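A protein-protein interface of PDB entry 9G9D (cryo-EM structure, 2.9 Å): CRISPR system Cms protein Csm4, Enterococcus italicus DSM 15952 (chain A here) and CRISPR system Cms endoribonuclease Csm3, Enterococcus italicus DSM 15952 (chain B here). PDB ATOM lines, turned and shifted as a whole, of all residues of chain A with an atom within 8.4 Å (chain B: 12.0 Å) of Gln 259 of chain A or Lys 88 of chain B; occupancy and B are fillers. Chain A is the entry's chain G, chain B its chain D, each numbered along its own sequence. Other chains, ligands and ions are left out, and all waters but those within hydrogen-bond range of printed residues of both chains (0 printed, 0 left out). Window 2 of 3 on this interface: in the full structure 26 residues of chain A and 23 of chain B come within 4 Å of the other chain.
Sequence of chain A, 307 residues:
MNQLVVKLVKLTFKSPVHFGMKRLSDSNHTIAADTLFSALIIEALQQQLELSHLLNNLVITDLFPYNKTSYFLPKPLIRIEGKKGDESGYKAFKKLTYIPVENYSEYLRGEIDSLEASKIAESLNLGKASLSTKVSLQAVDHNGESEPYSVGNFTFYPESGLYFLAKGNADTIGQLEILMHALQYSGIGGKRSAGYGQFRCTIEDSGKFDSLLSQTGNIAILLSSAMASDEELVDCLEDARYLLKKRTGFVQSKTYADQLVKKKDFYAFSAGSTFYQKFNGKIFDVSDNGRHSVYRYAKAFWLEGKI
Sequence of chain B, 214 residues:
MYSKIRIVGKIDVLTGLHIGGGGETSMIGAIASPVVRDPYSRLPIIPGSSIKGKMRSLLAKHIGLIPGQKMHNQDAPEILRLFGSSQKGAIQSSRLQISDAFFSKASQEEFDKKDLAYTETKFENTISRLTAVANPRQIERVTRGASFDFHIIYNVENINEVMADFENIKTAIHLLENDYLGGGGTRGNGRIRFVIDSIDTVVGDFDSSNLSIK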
ATOM      1  N   PHE A 250      36.409   7.010  23.953  1.00  0.00           N
ATOM      2  CA  PHE A 250      35.019   7.071  23.524  1.00  0.00           C
ATOM      3  C   PHE A 250      34.395   8.349  24.061  1.00  0.00           C
ATOM      4  O   PHE A 250      34.656   8.733  25.204  1.00  0.00           O
ATOM      5  CB  PHE A 250      34.232   5.863  24.026  1.00  0.00           C
ATOM      6  CG  PHE A 250      34.430   4.624  23.214  1.00  0.00           C
ATOM      7  CD1 PHE A 250      35.540   3.824  23.406  1.00  0.00           C
ATOM      8  CD2 PHE A 250      33.497   4.253  22.264  1.00  0.00           C
ATOM      9  CE1 PHE A 250      35.717   2.681  22.662  1.00  0.00           C
ATOM     10  CE2 PHE A 250      33.670   3.110  21.518  1.00  0.00           C
ATOM     11  CZ  PHE A 250      34.781   2.323  21.717  1.00  0.00           C
ATOM     12  N   VAL A 251      33.575   9.006  23.238  1.00  0.00           N
ATOM     13  CA  VAL A 251      32.849  10.177  23.710  1.00  0.00           C
ATOM     14  C   VAL A 251      31.929   9.769  24.851  1.00  0.00           C
ATOM     15  O   VAL A 251      31.300   8.702  24.819  1.00  0.00           O
ATOM     16  CB  VAL A 251      32.062  10.829  22.561  1.00  0.00           C
ATOM     17  CG1 VAL A 251      31.219  11.979  23.073  1.00  0.00           C
ATOM     18  CG2 VAL A 251      33.009  11.325  21.492  1.00  0.00           C
ATOM     19  N   SER A 253      28.837  11.328  26.415  1.00  0.00           N
ATOM     20  CA  SER A 253      27.754  12.296  26.452  1.00  0.00           C
ATOM     21  C   SER A 253      26.492  11.660  25.894  1.00  0.00           C
ATOM     22  O   SER A 253      26.547  10.695  25.127  1.00  0.00           O
ATOM     23  CB  SER A 253      28.089  13.563  25.661  1.00  0.00           C
ATOM     24  OG  SER A 253      27.033  14.502  25.759  1.00  0.00           O
ATOM     25  N   LYS A 254      25.350  12.216  26.297  1.00  0.00           N
ATOM     26  CA  LYS A 254      24.078  11.797  25.724  1.00  0.00           C
ATOM     27  C   LYS A 254      23.749  12.607  24.477  1.00  0.00           C
ATOM     28  O   LYS A 254      23.093  12.110  23.555  1.00  0.00           O
ATOM     29  CB  LYS A 254      22.974  11.939  26.770  1.00  0.00           C
ATOM     30  CG  LYS A 254      23.352  11.383  28.134  1.00  0.00           C
ATOM     31  CD  LYS A 254      22.339  11.770  29.197  1.00  0.00           C
ATOM     32  CE  LYS A 254      22.302  13.275  29.396  1.00  0.00           C
ATOM     33  NZ  LYS A 254      23.636  13.812  29.778  1.00  0.00           N
ATOM     34  N   THR A 255      24.209  13.859  24.431  1.00  0.00           N
ATOM     35  CA  THR A 255      23.847  14.753  23.337  1.00  0.00           C
ATOM     36  C   THR A 255      24.617  14.425  22.062  1.00  0.00           C
ATOM     37  O   THR A 255      24.138  14.697  20.955  1.00  0.00           O
ATOM     38  CB  THR A 255      24.096  16.205  23.753  1.00  0.00           C
ATOM     39  OG1 THR A 255      23.544  16.427  25.056  1.00  0.00           O
ATOM     40  CG2 THR A 255      23.448  17.170  22.771  1.00  0.00           C
ATOM     41  N   TYR A 256      25.809  13.835  22.198  1.00  0.00           N
ATOM     42  CA  TYR A 256      26.718  13.717  21.059  1.00  0.00           C
ATOM     43  C   TYR A 256      26.106  12.909  19.922  1.00  0.00           C
ATOM     44  O   TYR A 256      26.081  13.365  18.773  1.00  0.00           O
ATOM     45  CB  TYR A 256      28.038  13.090  21.507  1.00  0.00           C
ATOM     46  CG  TYR A 256      29.106  13.092  20.437  1.00  0.00           C
ATOM     47  CD1 TYR A 256      29.709  14.275  20.035  1.00  0.00           C
ATOM     48  CD2 TYR A 256      29.516  11.911  19.834  1.00  0.00           C
ATOM     49  CE1 TYR A 256      30.683  14.284  19.062  1.00  0.00           C
ATOM     50  CE2 TYR A 256      30.492  11.911  18.859  1.00  0.00           C
ATOM     51  CZ  TYR A 256      31.072  13.100  18.477  1.00  0.00           C
ATOM     52  OH  TYR A 256      32.044  13.107  17.506  1.00  0.00           O
ATOM     53  N   ALA A 257      25.607  11.713  20.216  1.00  0.00           N
ATOM     54  CA  ALA A 257      25.067  10.851  19.175  1.00  0.00           C
ATOM     55  C   ALA A 257      24.101   9.860  19.804  1.00  0.00           C
ATOM     56  O   ALA A 257      24.019   9.737  21.029  1.00  0.00           O
ATOM     57  CB  ALA A 257      26.181  10.116  18.422  1.00  0.00           C
ATOM     58  N   ASP A 258      23.359   9.159  18.942  1.00  0.00           N
ATOM     59  CA  ASP A 258      22.452   8.123  19.424  1.00  0.00           C
ATOM     60  C   ASP A 258      23.218   6.998  20.107  1.00  0.00           C
ATOM     61  O   ASP A 258      22.784   6.479  21.141  1.00  0.00           O
ATOM     62  CB  ASP A 258      21.611   7.581  18.268  1.00  0.00           C
ATOM     63  CG  ASP A 258      20.589   8.584  17.770  1.00  0.00           C
ATOM     64  OD1 ASP A 258      20.019   9.316  18.606  1.00  0.00           O
ATOM     65  OD2 ASP A 258      20.355   8.643  16.545  1.00  0.00           O
ATOM     66  N   GLN A 259      24.358   6.610  19.545  1.00  0.00           N
ATOM     67  CA  GLN A 259      25.228   5.600  20.128  1.00  0.00           C
ATOM     68  C   GLN A 259      26.601   6.204  20.383  1.00  0.00           C
ATOM     69  O   GLN A 259      26.986   7.185  19.739  1.00  0.00           O
ATOM     70  CB  GLN A 259      25.349   4.374  19.215  1.00  0.00           C
ATOM     71  CG  GLN A 259      25.874   4.678  17.823  1.00  0.00           C
ATOM     72  CD  GLN A 259      25.968   3.436  16.957  1.00  0.00           C
ATOM     73  OE1 GLN A 259      25.693   2.326  17.412  1.00  0.00           O
ATOM     74  NE2 GLN A 259      26.356   3.619  15.700  1.00  0.00           N
ATOM     75  N   LEU A 260      27.329   5.621  21.332  1.00  0.00           N
ATOM     76  CA  LEU A 260      28.632   6.153  21.708  1.00  0.00           C
ATOM     77  C   LEU A 260      29.621   6.025  20.554  1.00  0.00           C
ATOM     78  O   LEU A 260      29.698   4.990  19.888  1.00  0.00           O
ATOM     79  CB  LEU A 260      29.156   5.426  22.945  1.00  0.00           C
ATOM     80  CG  LEU A 260      28.224   5.477  24.158  1.00  0.00           C
ATOM     81  CD1 LEU A 260      28.770   4.628  25.285  1.00  0.00           C
ATOM     82  CD2 LEU A 260      28.018   6.909  24.620  1.00  0.00           C
ATOM     83  N   VAL A 261      30.383   7.093  20.325  1.00  0.00           N
ATOM     84  CA  VAL A 261      31.300   7.204  19.198  1.00  0.00           C
ATOM     85  C   VAL A 261      32.691   7.516  19.729  1.00  0.00           C
ATOM     86  O   VAL A 261      32.844   8.312  20.661  1.00  0.00           O
ATOM     87  CB  VAL A 261      30.835   8.292  18.207  1.00  0.00           C
ATOM     88  CG1 VAL A 261      31.829   8.447  17.070  1.00  0.00           C
ATOM     89  CG2 VAL A 261      29.456   7.961  17.669  1.00  0.00           C
ATOM     90  N   LYS A 262      33.704   6.880  19.142  1.00  0.00           N
ATOM     91  CA  LYS A 262      35.080   7.138  19.547  1.00  0.00           C
ATOM     92  C   LYS A 262      35.497   8.559  19.188  1.00  0.00           C
ATOM     93  O   LYS A 262      35.044   9.126  18.191  1.00  0.00           O
ATOM     94  CB  LYS A 262      36.029   6.139  18.882  1.00  0.00           C
ATOM     95  CG  LYS A 262      35.955   4.739  19.447  1.00  0.00           C
ATOM     96  CD  LYS A 262      36.986   3.833  18.802  1.00  0.00           C
ATOM     97  CE  LYS A 262      38.392   4.349  19.032  1.00  0.00           C
ATOM     98  NZ  LYS A 262      38.717   4.414  20.479  1.00  0.00           N
ATOM     99  N   ARG A 291      26.958  16.018  17.245  1.00  0.00           N
ATOM    100  CA  ARG A 291      26.047  17.128  17.512  1.00  0.00           C
ATOM    101  C   ARG A 291      26.747  18.259  18.257  1.00  0.00           C
ATOM    102  O   ARG A 291      26.445  19.436  18.035  1.00  0.00           O
ATOM    103  CB  ARG A 291      24.828  16.636  18.289  1.00  0.00           C
ATOM    104  CG  ARG A 291      23.868  15.806  17.449  1.00  0.00           C
ATOM    105  CD  ARG A 291      22.491  15.720  18.081  1.00  0.00           C
ATOM    106  NE  ARG A 291      22.412  14.691  19.110  1.00  0.00           N
ATOM    107  CZ  ARG A 291      22.039  13.438  18.887  1.00  0.00           C
ATOM    108  NH1 ARG A 291      21.722  13.017  17.673  1.00  0.00           N
ATOM    109  NH2 ARG A 291      21.981  12.586  19.907  1.00  0.00           N
ATOM    110  N   ARG B  56      19.143  -2.774  41.493  1.00  0.00           N
ATOM    111  CA  ARG B  56      18.595  -2.775  40.140  1.00  0.00           C
ATOM    112  C   ARG B  56      17.847  -4.073  39.847  1.00  0.00           C
ATOM    113  O   ARG B  56      16.772  -4.060  39.240  1.00  0.00           O
ATOM    114  CB  ARG B  56      19.720  -2.552  39.128  1.00  0.00           C
ATOM    115  CG  ARG B  56      19.272  -2.461  37.677  1.00  0.00           C
ATOM    116  CD  ARG B  56      20.473  -2.533  36.742  1.00  0.00           C
ATOM    117  NE  ARG B  56      20.101  -2.523  35.332  1.00  0.00           N
ATOM    118  CZ  ARG B  56      20.200  -1.469  34.535  1.00  0.00           C
ATOM    119  NH1 ARG B  56      20.650  -0.307  34.976  1.00  0.00           N
ATOM    120  NH2 ARG B  56      19.847  -1.583  33.259  1.00  0.00           N
ATOM    121  N   GLN B  74      17.169  -3.013  33.193  1.00  0.00           N
ATOM    122  CA  GLN B  74      16.159  -3.679  32.382  1.00  0.00           C
ATOM    123  C   GLN B  74      15.378  -2.677  31.542  1.00  0.00           C
ATOM    124  O   GLN B  74      15.682  -1.489  31.533  1.00  0.00           O
ATOM    125  CB  GLN B  74      15.208  -4.486  33.268  1.00  0.00           C
ATOM    126  CG  GLN B  74      15.710  -5.886  33.616  1.00  0.00           C
ATOM    127  CD  GLN B  74      16.985  -5.883  34.444  1.00  0.00           C
ATOM    128  OE1 GLN B  74      17.345  -4.879  35.060  1.00  0.00           O
ATOM    129  NE2 GLN B  74      17.677  -7.016  34.460  1.00  0.00           N
ATOM    130  N   ASP B  75      14.359  -3.176  30.840  1.00  0.00           N
ATOM    131  CA  ASP B  75      13.657  -2.358  29.855  1.00  0.00           C
ATOM    132  C   ASP B  75      12.962  -1.162  30.494  1.00  0.00           C
ATOM    133  O   ASP B  75      12.798  -0.117  29.852  1.00  0.00           O
ATOM    134  CB  ASP B  75      12.646  -3.217  29.094  1.00  0.00           C
ATOM    135  CG  ASP B  75      11.898  -2.436  28.032  1.00  0.00           C
ATOM    136  OD1 ASP B  75      12.519  -2.067  27.014  1.00  0.00           O
ATOM    137  OD2 ASP B  75      10.686  -2.193  28.214  1.00  0.00           O
ATOM    138  N   LEU B  80      16.074   2.062  34.473  1.00  0.00           N
ATOM    139  CA  LEU B  80      17.160   2.424  33.532  1.00  0.00           C
ATOM    140  C   LEU B  80      17.694   3.832  33.835  1.00  0.00           C
ATOM    141  O   LEU B  80      18.925   4.002  33.823  1.00  0.00           O
ATOM    142  CB  LEU B  80      16.558   2.352  32.132  1.00  0.00           C
ATOM    143  CG  LEU B  80      17.483   1.879  31.011  1.00  0.00           C
ATOM    144  CD1 LEU B  80      18.244   0.641  31.435  1.00  0.00           C
ATOM    145  CD2 LEU B  80      16.669   1.598  29.762  1.00  0.00           C
ATOM    146  N   GLY B  84      21.461   4.019  35.080  1.00  0.00           N
ATOM    147  CA  GLY B  84      22.282   4.216  33.894  1.00  0.00           C
ATOM    148  C   GLY B  84      21.832   3.377  32.717  1.00  0.00           C
ATOM    149  O   GLY B  84      21.424   2.225  32.849  1.00  0.00           O
ATOM    150  N   SER B  85      21.924   3.976  31.531  1.00  0.00           N
ATOM    151  CA  SER B  85      21.537   3.334  30.283  1.00  0.00           C
ATOM    152  C   SER B  85      22.544   3.687  29.202  1.00  0.00           C
ATOM    153  O   SER B  85      22.929   4.851  29.068  1.00  0.00           O
ATOM    154  CB  SER B  85      20.138   3.774  29.847  1.00  0.00           C
ATOM    155  OG  SER B  85      19.775   3.182  28.613  1.00  0.00           O
ATOM    156  N   SER B  86      22.942   2.691  28.414  1.00  0.00           N
ATOM    157  CA  SER B  86      23.847   2.904  27.295  1.00  0.00           C
ATOM    158  C   SER B  86      23.258   2.445  25.967  1.00  0.00           C
ATOM    159  O   SER B  86      23.992   2.340  24.979  1.00  0.00           O
ATOM    160  CB  SER B  86      25.170   2.191  27.553  1.00  0.00           C
ATOM    161  OG  SER B  86      26.068   2.379  26.476  1.00  0.00           O
ATOM    162  N   GLN B  87      21.957   2.168  25.924  1.00  0.00           N
ATOM    163  CA  GLN B  87      21.315   1.732  24.692  1.00  0.00           C
ATOM    164  C   GLN B  87      21.336   2.847  23.655  1.00  0.00           C
ATOM    165  O   GLN B  87      21.266   4.034  23.985  1.00  0.00           O
ATOM    166  CB  GLN B  87      19.876   1.302  24.968  1.00  0.00           C
ATOM    167  CG  GLN B  87      19.743   0.221  26.023  1.00  0.00           C
ATOM    168  CD  GLN B  87      18.299  -0.094  26.355  1.00  0.00           C
ATOM    169  OE1 GLN B  87      17.378   0.472  25.767  1.00  0.00           O
ATOM    170  NE2 GLN B  87      18.093  -1.002  27.304  1.00  0.00           N
ATOM    171  N   LYS B  88      21.429   2.453  22.385  1.00  0.00           N
ATOM    172  CA  LYS B  88      21.481   3.426  21.302  1.00  0.00           C
ATOM    173  C   LYS B  88      20.213   4.269  21.284  1.00  0.00           C
ATOM    174  O   LYS B  88      19.098   3.740  21.300  1.00  0.00           O
ATOM    175  CB  LYS B  88      21.673   2.720  19.960  1.00  0.00           C
ATOM    176  CG  LYS B  88      20.761   1.527  19.739  1.00  0.00           C
ATOM    177  CD  LYS B  88      20.893   0.996  18.322  1.00  0.00           C
ATOM    178  CE  LYS B  88      22.327   0.598  18.010  1.00  0.00           C
ATOM    179  NZ  LYS B  88      22.467   0.098  16.615  1.00  0.00           N
ATOM    180  N   GLY B  89      20.389   5.589  21.255  1.00  0.00           N
ATOM    181  CA  GLY B  89      19.279   6.514  21.302  1.00  0.00           C
ATOM    182  C   GLY B  89      18.702   6.749  22.678  1.00  0.00           C
ATOM    183  O   GLY B  89      17.824   7.608  22.825  1.00  0.00           O
ATOM    184  N   ALA B  90      19.164   6.020  23.691  1.00  0.00           N
ATOM    185  CA  ALA B  90      18.660   6.124  25.056  1.00  0.00           C
ATOM    186  C   ALA B  90      19.815   6.176  26.045  1.00  0.00           C
ATOM    187  O   ALA B  90      19.845   5.462  27.049  1.00  0.00           O
ATOM    188  CB  ALA B  90      17.720   4.965  25.376  1.00  0.00           C
ATOM    189  N   ILE B  91      20.798   7.027  25.762  1.00  0.00           N
ATOM    190  CA  ILE B  91      21.940   7.197  26.656  1.00  0.00           C
ATOM    191  C   ILE B  91      21.472   7.990  27.873  1.00  0.00           C
ATOM    192  O   ILE B  91      21.043   9.139  27.748  1.00  0.00           O
ATOM    193  CB  ILE B  91      23.109   7.896  25.953  1.00  0.00           C
ATOM    194  CG1 ILE B  91      23.494   7.142  24.678  1.00  0.00           C
ATOM    195  CG2 ILE B  91      24.301   8.003  26.885  1.00  0.00           C
ATOM    196  CD1 ILE B  91      24.009   5.750  24.930  1.00  0.00           C
ATOM    197  N   GLN B  92      21.544   7.374  29.051  1.00  0.00           N
ATOM    198  CA  GLN B  92      21.110   7.991  30.298  1.00  0.00           C
ATOM    199  C   GLN B  92      22.219   7.842  31.325  1.00  0.00           C
ATOM    200  O   GLN B  92      22.770   6.749  31.491  1.00  0.00           O
ATOM    201  CB  GLN B  92      19.817   7.351  30.812  1.00  0.00           C
ATOM    202  CG  GLN B  92      18.594   7.644  29.965  1.00  0.00           C
ATOM    203  CD  GLN B  92      17.370   6.894  30.443  1.00  0.00           C
ATOM    204  OE1 GLN B  92      17.399   5.675  30.607  1.00  0.00           O
ATOM    205  NE2 GLN B  92      16.284   7.622  30.676  1.00  0.00           N
ATOM    206  N   SER B  93      22.549   8.936  32.004  1.00  0.00           N
ATOM    207  CA  SER B  93      23.514   8.876  33.092  1.00  0.00           C
ATOM    208  C   SER B  93      22.886   8.225  34.317  1.00  0.00           C
ATOM    209  O   SER B  93      21.712   8.446  34.622  1.00  0.00           O
ATOM    210  CB  SER B  93      24.011  10.279  33.438  1.00  0.00           C
ATOM    211  OG  SER B  93      24.588  10.908  32.307  1.00  0.00           O
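The backbone NH (N) of Gly 89 of chain B is in hydrogen-bond range of the backbone carbonyl oxygen (O) of Asp 258 of chain A, 2.6 Å away.
OG of Ser 253 of chain A sits at hydrogen-bond distance from N of Thr 255 of chain A (3.2 Å).
Among the printed residues, pairs that only touch across the chains: Ser 253 of chain A with Ile 91 of chain B (3.9 Å), Lys 254 of chain A with Ile 91 of chain B (3.2 Å), Lys 254 of chain A with Ser 93 of chain B (3.9 Å), Asp 258 of chain A with Lys 88 of chain B (3.3 Å), Asp 258 of chain A with Ile 91 of chain B (3.7 Å), Gln 259 of chain A with Lys 88 of chain B (3.8 Å) and Leu 260 of chain A with Ser 86 of chain B (3.7 Å).
No residue of chain B comes within 4 Å of Val 251 of chain A. Printed residues of chain B within 4 Å of Ser 253 of chain A: Ile 91. Printed residues of chain B within 4 Å of Lys 254 of chain A: Ile 91 and Ser 93. No residue of chain B comes within 4 Å of Ala 257 of chain A. Asp 258 of chain A touches just these residues of chain B: Lys 88 (3.3 Å), Gly 89 (2.6 Å) and Ile 91 (3.7 Å). Of chain B, only Lys 88 (3.8 Å) comes within 4 Å of Gln 259 of chain A. Printed residues of chain B within 4 Å of Leu 260 of chain A: Ser 86 (3.7 Å). No residue of chain B comes within 4 Å of Val 261 of chain A. Lys 88 of chain B touches two residues of chain A. Of chain A, only Asp 258 comes within 4 Å of Gly 89 of chain B. The nearest residue of chain B that does not touch Gln 259 of chain A is Gly 89 of chain B (4.4 Å). The nearest residue of chain A that does not touch Lys 88 of chain B is Leu 260 of chain A (6.2 Å).
Printed residues of chain A that touch a printed residue of chain B: Ser 253, Lys 254, Asp 258, Gln 259 and Leu 260. Hydrophobic or aromatic side chains of chain A within 4 Å of the printed part of chain B: Leu 260.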
